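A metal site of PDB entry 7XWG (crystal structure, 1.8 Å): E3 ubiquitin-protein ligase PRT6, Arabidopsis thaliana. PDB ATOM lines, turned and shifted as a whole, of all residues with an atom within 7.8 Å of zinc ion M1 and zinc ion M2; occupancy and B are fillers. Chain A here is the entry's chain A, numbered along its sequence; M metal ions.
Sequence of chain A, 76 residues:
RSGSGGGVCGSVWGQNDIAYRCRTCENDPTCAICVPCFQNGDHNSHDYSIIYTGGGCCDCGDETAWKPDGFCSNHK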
ATOM      1  N   GLY A   7     -20.065  22.545  -7.555  1.00  0.00           N
ATOM      2  CA  GLY A   7     -21.199  23.439  -7.712  1.00  0.00           C
ATOM      3  C   GLY A   7     -21.366  24.393  -6.544  1.00  0.00           C
ATOM      4  O   GLY A   7     -21.163  24.023  -5.379  1.00  0.00           O
ATOM      5  N   VAL A   8     -21.691  25.634  -6.844  1.00  0.00           N
ATOM      6  CA  VAL A   8     -21.949  26.703  -5.880  1.00  0.00           C
ATOM      7  C   VAL A   8     -23.427  26.700  -5.456  1.00  0.00           C
ATOM      8  O   VAL A   8     -24.324  26.519  -6.294  1.00  0.00           O
ATOM      9  CB  VAL A   8     -21.533  28.045  -6.498  1.00  0.00           C
ATOM     10  CG1 VAL A   8     -21.682  29.157  -5.517  1.00  0.00           C
ATOM     11  CG2 VAL A   8     -20.103  27.922  -7.008  1.00  0.00           C
ATOM     12  N   CYS A   9     -23.703  26.914  -4.164  1.00  0.00           N
ATOM     13  CA  CYS A   9     -25.059  27.134  -3.689  1.00  0.00           C
ATOM     14  C   CYS A   9     -25.659  28.435  -4.192  1.00  0.00           C
ATOM     15  O   CYS A   9     -25.021  29.500  -4.098  1.00  0.00           O
ATOM     16  CB  CYS A   9     -25.022  27.093  -2.134  1.00  0.00           C
ATOM     17  SG  CYS A   9     -26.603  27.612  -1.171  1.00  0.00           S
ATOM     18  N   GLY A  10     -26.895  28.364  -4.680  1.00  0.00           N
ATOM     19  CA  GLY A  10     -27.604  29.522  -5.167  1.00  0.00           C
ATOM     20  C   GLY A  10     -28.558  30.155  -4.165  1.00  0.00           C
ATOM     21  O   GLY A  10     -29.402  30.983  -4.552  1.00  0.00           O
ATOM     22  N   SER A  11     -28.448  29.795  -2.895  1.00  0.00           N
ATOM     23  CA  SER A  11     -29.388  30.311  -1.915  1.00  0.00           C
ATOM     24  C   SER A  11     -29.113  31.787  -1.620  1.00  0.00           C
ATOM     25  O   SER A  11     -28.021  32.303  -1.782  1.00  0.00           O
ATOM     26  CB  SER A  11     -29.303  29.511  -0.624  1.00  0.00           C
ATOM     27  OG  SER A  11     -30.179  28.424  -0.677  1.00  0.00           O
ATOM     28  N   VAL A  12     -30.129  32.421  -1.085  1.00  0.00           N
ATOM     29  CA  VAL A  12     -30.162  33.863  -0.993  1.00  0.00           C
ATOM     30  C   VAL A  12     -30.864  34.205   0.301  1.00  0.00           C
ATOM     31  O   VAL A  12     -31.655  33.408   0.809  1.00  0.00           O
ATOM     32  CB  VAL A  12     -30.898  34.381  -2.252  1.00  0.00           C
ATOM     33  CG1 VAL A  12     -31.523  35.580  -1.972  1.00  0.00           C
ATOM     34  CG2 VAL A  12     -29.945  34.488  -3.424  1.00  0.00           C
ATOM     35  N   TRP A  13     -30.553  35.361   0.867  1.00  0.00           N
ATOM     36  CA  TRP A  13     -31.371  35.835   1.979  1.00  0.00           C
ATOM     37  C   TRP A  13     -31.604  37.339   1.871  1.00  0.00           C
ATOM     38  O   TRP A  13     -30.896  38.058   1.154  1.00  0.00           O
ATOM     39  CB  TRP A  13     -30.765  35.487   3.343  1.00  0.00           C
ATOM     40  CG  TRP A  13     -29.408  36.012   3.563  1.00  0.00           C
ATOM     41  CD1 TRP A  13     -29.053  37.202   4.144  1.00  0.00           C
ATOM     42  CD2 TRP A  13     -28.184  35.365   3.204  1.00  0.00           C
ATOM     43  NE1 TRP A  13     -27.664  37.331   4.154  1.00  0.00           N
ATOM     44  CE2 TRP A  13     -27.118  36.213   3.567  1.00  0.00           C
ATOM     45  CE3 TRP A  13     -27.887  34.157   2.572  1.00  0.00           C
ATOM     46  CZ2 TRP A  13     -25.770  35.870   3.352  1.00  0.00           C
ATOM     47  CZ3 TRP A  13     -26.549  33.813   2.360  1.00  0.00           C
ATOM     48  CH2 TRP A  13     -25.509  34.678   2.743  1.00  0.00           C
ATOM     49  N   ALA A  32     -20.155  34.992   3.521  1.00  0.00           N
ATOM     50  CA  ALA A  32     -21.174  34.434   4.398  1.00  0.00           C
ATOM     51  C   ALA A  32     -21.841  33.275   3.682  1.00  0.00           C
ATOM     52  O   ALA A  32     -21.834  33.195   2.445  1.00  0.00           O
ATOM     53  CB  ALA A  32     -22.170  35.511   4.799  1.00  0.00           C
ATOM     54  N   ILE A  33     -22.424  32.370   4.468  1.00  0.00           N
ATOM     55  CA  ILE A  33     -23.157  31.218   3.937  1.00  0.00           C
ATOM     56  C   ILE A  33     -24.515  31.108   4.625  1.00  0.00           C
ATOM     57  O   ILE A  33     -24.699  31.603   5.738  1.00  0.00           O
ATOM     58  CB  ILE A  33     -22.362  29.910   4.133  1.00  0.00           C
ATOM     59  CG1 ILE A  33     -22.090  29.661   5.605  1.00  0.00           C
ATOM     60  CG2 ILE A  33     -21.027  30.014   3.406  1.00  0.00           C
ATOM     61  CD1 ILE A  33     -21.450  28.286   5.887  1.00  0.00           C
ATOM     62  N   CYS A  34     -25.472  30.475   3.926  1.00  0.00           N
ATOM     63  CA  CYS A  34     -26.820  30.303   4.467  1.00  0.00           C
ATOM     64  C   CYS A  34     -26.825  29.327   5.629  1.00  0.00           C
ATOM     65  O   CYS A  34     -25.883  28.560   5.850  1.00  0.00           O
ATOM     66  CB  CYS A  34     -27.794  29.814   3.376  1.00  0.00           C
ATOM     67  SG  CYS A  34     -27.431  28.130   2.740  1.00  0.00           S
ATOM     68  N   VAL A  35     -27.892  29.370   6.408  1.00  0.00           N
ATOM     69  CA  VAL A  35     -27.967  28.513   7.583  1.00  0.00           C
ATOM     70  C   VAL A  35     -27.871  27.037   7.224  1.00  0.00           C
ATOM     71  O   VAL A  35     -27.131  26.316   7.901  1.00  0.00           O
ATOM     72  CB  VAL A  35     -29.218  28.853   8.405  1.00  0.00           C
ATOM     73  CG1 VAL A  35     -29.426  27.820   9.513  1.00  0.00           C
ATOM     74  CG2 VAL A  35     -29.055  30.251   8.946  1.00  0.00           C
ATOM     75  N   PRO A  36     -28.615  26.514   6.243  1.00  0.00           N
ATOM     76  CA  PRO A  36     -28.484  25.079   5.935  1.00  0.00           C
ATOM     77  C   PRO A  36     -27.058  24.693   5.529  1.00  0.00           C
ATOM     78  O   PRO A  36     -26.556  23.642   5.937  1.00  0.00           O
ATOM     79  CB  PRO A  36     -29.491  24.862   4.791  1.00  0.00           C
ATOM     80  CG  PRO A  36     -30.515  25.968   4.993  1.00  0.00           C
ATOM     81  CD  PRO A  36     -29.732  27.143   5.519  1.00  0.00           C
ATOM     82  N   CYS A  37     -26.397  25.535   4.741  1.00  0.00           N
ATOM     83  CA  CYS A  37     -25.018  25.246   4.381  1.00  0.00           C
ATOM     84  C   CYS A  37     -24.129  25.211   5.604  1.00  0.00           C
ATOM     85  O   CYS A  37     -23.278  24.316   5.738  1.00  0.00           O
ATOM     86  CB  CYS A  37     -24.539  26.275   3.352  1.00  0.00           C
ATOM     87  SG  CYS A  37     -25.139  25.863   1.724  1.00  0.00           S
ATOM     88  N   PHE A  38     -24.294  26.162   6.525  1.00  0.00           N
ATOM     89  CA  PHE A  38     -23.542  26.117   7.779  1.00  0.00           C
ATOM     90  C   PHE A  38     -23.855  24.848   8.568  1.00  0.00           C
ATOM     91  O   PHE A  38     -22.947  24.178   9.066  1.00  0.00           O
ATOM     92  CB  PHE A  38     -23.830  27.361   8.608  1.00  0.00           C
ATOM     93  CG  PHE A  38     -23.064  27.417   9.902  1.00  0.00           C
ATOM     94  CD1 PHE A  38     -21.820  28.031   9.967  1.00  0.00           C
ATOM     95  CD2 PHE A  38     -23.578  26.832  11.046  1.00  0.00           C
ATOM     96  CE1 PHE A  38     -21.128  28.070  11.131  1.00  0.00           C
ATOM     97  CE2 PHE A  38     -22.869  26.861  12.224  1.00  0.00           C
ATOM     98  CZ  PHE A  38     -21.647  27.488  12.262  1.00  0.00           C
ATOM     99  N   ASN A  40     -24.817  21.980   7.558  1.00  0.00           N
ATOM    100  CA  ASN A  40     -24.343  20.777   6.887  1.00  0.00           C
ATOM    101  C   ASN A  40     -22.834  20.770   6.710  1.00  0.00           C
ATOM    102  O   ASN A  40     -22.315  19.933   5.964  1.00  0.00           O
ATOM    103  CB  ASN A  40     -25.014  20.629   5.532  1.00  0.00           C
ATOM    104  CG  ASN A  40     -26.462  20.217   5.644  1.00  0.00           C
ATOM    105  OD1 ASN A  40     -26.815  19.381   6.470  1.00  0.00           O
ATOM    106  ND2 ASN A  40     -27.311  20.801   4.792  1.00  0.00           N
ATOM    107  N   GLY A  41     -22.126  21.679   7.351  1.00  0.00           N
ATOM    108  CA  GLY A  41     -20.683  21.666   7.356  1.00  0.00           C
ATOM    109  C   GLY A  41     -20.194  21.479   8.765  1.00  0.00           C
ATOM    110  O   GLY A  41     -20.991  21.274   9.678  1.00  0.00           O
ATOM    111  N   CYS A  57     -25.984  36.582  -0.982  1.00  0.00           N
ATOM    112  CA  CYS A  57     -25.924  35.317  -1.673  1.00  0.00           C
ATOM    113  C   CYS A  57     -24.902  34.435  -0.961  1.00  0.00           C
ATOM    114  O   CYS A  57     -23.824  34.903  -0.578  1.00  0.00           O
ATOM    115  CB  CYS A  57     -25.488  35.521  -3.131  1.00  0.00           C
ATOM    116  SG  CYS A  57     -26.681  36.412  -4.162  1.00  0.00           S
ATOM    117  N   CYS A  58     -25.242  33.158  -0.855  1.00  0.00           N
ATOM    118  CA  CYS A  58     -24.431  32.196  -0.131  1.00  0.00           C
ATOM    119  C   CYS A  58     -23.158  31.904  -0.906  1.00  0.00           C
ATOM    120  O   CYS A  58     -23.196  31.702  -2.122  1.00  0.00           O
ATOM    121  CB  CYS A  58     -25.224  30.909   0.104  1.00  0.00           C
ATOM    122  SG  CYS A  58     -24.363  29.584   0.999  1.00  0.00           S
ATOM    123  N   ASP A  59     -22.022  31.929  -0.224  1.00  0.00           N
ATOM    124  CA  ASP A  59     -20.721  31.654  -0.845  1.00  0.00           C
ATOM    125  C   ASP A  59     -20.278  30.176  -0.737  1.00  0.00           C
ATOM    126  O   ASP A  59     -19.141  29.854  -1.133  1.00  0.00           O
ATOM    127  CB  ASP A  59     -19.694  32.562  -0.203  1.00  0.00           C
ATOM    128  CG  ASP A  59     -19.991  34.016  -0.482  1.00  0.00           C
ATOM    129  OD1 ASP A  59     -20.270  34.333  -1.639  1.00  0.00           O
ATOM    130  OD2 ASP A  59     -19.983  34.833   0.471  1.00  0.00           O
ATOM    131  N   CYS A  60     -21.149  29.279  -0.276  1.00  0.00           N
ATOM    132  CA  CYS A  60     -20.772  27.877  -0.090  1.00  0.00           C
ATOM    133  C   CYS A  60     -20.468  27.258  -1.449  1.00  0.00           C
ATOM    134  O   CYS A  60     -21.283  27.337  -2.375  1.00  0.00           O
ATOM    135  CB  CYS A  60     -21.891  27.101   0.615  1.00  0.00           C
ATOM    136  SG  CYS A  60     -21.443  25.378   1.112  1.00  0.00           S
ATOM    137  N   GLY A  61     -19.281  26.642  -1.558  1.00  0.00           N
ATOM    138  CA  GLY A  61     -18.820  26.035  -2.793  1.00  0.00           C
ATOM    139  C   GLY A  61     -18.051  26.965  -3.709  1.00  0.00           C
ATOM    140  O   GLY A  61     -17.588  26.515  -4.766  1.00  0.00           O
ATOM    141  N   TRP A  66     -14.761  31.244  -0.047  1.00  0.00           N
ATOM    142  CA  TRP A  66     -14.878  30.338   1.086  1.00  0.00           C
ATOM    143  C   TRP A  66     -13.866  29.233   0.911  1.00  0.00           C
ATOM    144  O   TRP A  66     -13.727  28.711  -0.184  1.00  0.00           O
ATOM    145  CB  TRP A  66     -16.254  29.712   1.127  1.00  0.00           C
ATOM    146  CG  TRP A  66     -16.780  29.360   2.462  1.00  0.00           C
ATOM    147  CD1 TRP A  66     -16.916  28.115   2.963  1.00  0.00           C
ATOM    148  CD2 TRP A  66     -17.293  30.256   3.465  1.00  0.00           C
ATOM    149  NE1 TRP A  66     -17.465  28.165   4.218  1.00  0.00           N
ATOM    150  CE2 TRP A  66     -17.714  29.470   4.547  1.00  0.00           C
ATOM    151  CE3 TRP A  66     -17.420  31.641   3.547  1.00  0.00           C
ATOM    152  CZ2 TRP A  66     -18.267  30.018   5.711  1.00  0.00           C
ATOM    153  CZ3 TRP A  66     -17.974  32.203   4.713  1.00  0.00           C
ATOM    154  CH2 TRP A  66     -18.396  31.384   5.782  1.00  0.00           C
ATOM    155  N   GLY A  70     -14.528  24.451   4.461  1.00  0.00           N
ATOM    156  CA  GLY A  70     -15.758  24.995   4.991  1.00  0.00           C
ATOM    157  C   GLY A  70     -16.976  24.781   4.137  1.00  0.00           C
ATOM    158  O   GLY A  70     -18.078  25.224   4.516  1.00  0.00           O
ATOM    159  N   PHE A  71     -16.842  24.093   3.008  1.00  0.00           N
ATOM    160  CA  PHE A  71     -17.992  23.742   2.193  1.00  0.00           C
ATOM    161  C   PHE A  71     -18.888  22.767   2.937  1.00  0.00           C
ATOM    162  O   PHE A  71     -18.409  21.897   3.675  1.00  0.00           O
ATOM    163  CB  PHE A  71     -17.539  23.093   0.890  1.00  0.00           C
ATOM    164  CG  PHE A  71     -16.805  24.018  -0.037  1.00  0.00           C
ATOM    165  CD1 PHE A  71     -16.194  23.502  -1.176  1.00  0.00           C
ATOM    166  CD2 PHE A  71     -16.726  25.370   0.209  1.00  0.00           C
ATOM    167  CE1 PHE A  71     -15.510  24.329  -2.060  1.00  0.00           C
ATOM    168  CE2 PHE A  71     -16.068  26.220  -0.683  1.00  0.00           C
ATOM    169  CZ  PHE A  71     -15.452  25.688  -1.812  1.00  0.00           C
ATOM    170  N   CYS A  72     -20.200  22.909   2.759  1.00  0.00           N
ATOM    171  CA  CYS A  72     -21.155  21.928   3.263  1.00  0.00           C
ATOM    172  C   CYS A  72     -21.029  20.635   2.474  1.00  0.00           C
ATOM    173  O   CYS A  72     -20.352  20.562   1.437  1.00  0.00           O
ATOM    174  CB  CYS A  72     -22.585  22.497   3.234  1.00  0.00           C
ATOM    175  SG  CYS A  72     -23.497  22.273   1.772  1.00  0.00           S
ATOM    176  N   SER A  73     -21.670  19.595   2.983  1.00  0.00           N
ATOM    177  CA  SER A  73     -21.640  18.275   2.375  1.00  0.00           C
ATOM    178  C   SER A  73     -22.303  18.217   1.006  1.00  0.00           C
ATOM    179  O   SER A  73     -22.152  17.207   0.315  1.00  0.00           O
ATOM    180  CB  SER A  73     -22.281  17.265   3.335  1.00  0.00           C
ATOM    181  OG  SER A  73     -23.684  17.472   3.472  1.00  0.00           O
ATOM    182  N   ASN A  74     -23.013  19.253   0.577  1.00  0.00           N
ATOM    183  CA  ASN A  74     -23.746  19.205  -0.681  1.00  0.00           C
ATOM    184  C   ASN A  74     -23.160  20.078  -1.781  1.00  0.00           C
ATOM    185  O   ASN A  74     -23.701  20.095  -2.887  1.00  0.00           O
ATOM    186  CB  ASN A  74     -25.215  19.596  -0.466  1.00  0.00           C
ATOM    187  CG  ASN A  74     -25.947  18.670   0.498  1.00  0.00           C
ATOM    188  OD1 ASN A  74     -25.784  17.446   0.445  1.00  0.00           O
ATOM    189  ND2 ASN A  74     -26.746  19.253   1.381  1.00  0.00           N
ATOM    190  N   HIS A  75     -22.083  20.825  -1.513  1.00  0.00           N
ATOM    191  CA  HIS A  75     -21.464  21.711  -2.507  1.00  0.00           C
ATOM    192  C   HIS A  75     -19.958  21.441  -2.579  1.00  0.00           C
ATOM    193  O   HIS A  75     -19.166  22.210  -2.014  1.00  0.00           O
ATOM    194  CB  HIS A  75     -21.786  23.212  -2.216  1.00  0.00           C
ATOM    195  CG  HIS A  75     -23.249  23.483  -2.144  1.00  0.00           C
ATOM    196  ND1 HIS A  75     -23.874  23.823  -0.969  1.00  0.00           N
ATOM    197  CD2 HIS A  75     -24.214  23.424  -3.085  1.00  0.00           C
ATOM    198  CE1 HIS A  75     -25.182  23.921  -1.181  1.00  0.00           C
ATOM    199  NE2 HIS A  75     -25.403  23.718  -2.470  1.00  0.00           N
ATOM    200  N   LYS A  76     -19.579  20.406  -3.326  1.00  0.00           N
ATOM    201  CA  LYS A  76     -18.193  19.911  -3.472  1.00  0.00           C
ATOM    202  C   LYS A  76     -17.791  18.981  -2.314  1.00  0.00           C
ATOM    203  O   LYS A  76     -18.357  19.020  -1.209  1.00  0.00           O
ATOM    204  CB  LYS A  76     -17.189  21.074  -3.556  1.00  0.00           C
ATOM    205  CG  LYS A  76     -16.824  21.573  -4.949  1.00  0.00           C
ATOM    206  CD  LYS A  76     -17.653  22.820  -5.328  1.00  0.00           C
ATOM    207  CE  LYS A  76     -17.094  23.539  -6.552  1.00  0.00           C
ATOM    208  NZ  LYS A  76     -17.265  22.734  -7.804  1.00  0.00           N
HETATM  209 ZN    ZN M   1     -25.911  27.936   1.026  1.00  0.00          ZN
HETATM  210 ZN    ZN M   2     -23.365  24.415   0.883  1.00  0.00          ZN
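Four residues have an atom within 4 Å of zinc ion M1: Cys 9, Cys 34, Cys 37 and Cys 58.
Zinc ion M1 is bound by the side-chain sulfur of Cys 58, the side-chain sulfur of Cys 34, the side-chain sulfur of Cys 37 and the side-chain sulfur of Cys 9.
Zinc ion M2 is bound by a ring nitrogen (ND1) of His 75, the side-chain sulfur (SG) of Cys 60, the side-chain sulfur (SG) of Cys 72 and the side-chain sulfur (SG) of Cys 37.
Zinc ion M2 has four donor atoms within binding distance.
Along chain A the residues within 4 Å of zinc ion M2 span positions 37 to 75.
The backbone NH of Asn 74 sits close to the side-chain sulfur of Cys 72 (3.3 Å).
The backbone carbonyl oxygen (O) of Cys 60 is in hydrogen-bond range of the backbone NH (N) of Cys 9 (3.0 Å).
The side-chain sulfur (SG) of Cys 9 sits close to the backbone NH (N) of Ser 11, 3.3 Å away.
N of Cys 60 lies close to SG of Cys 58, at 3.5 Å.
O of Ser 11 lies within hydrogen-bond range of N of Cys 58 (3.1 Å).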
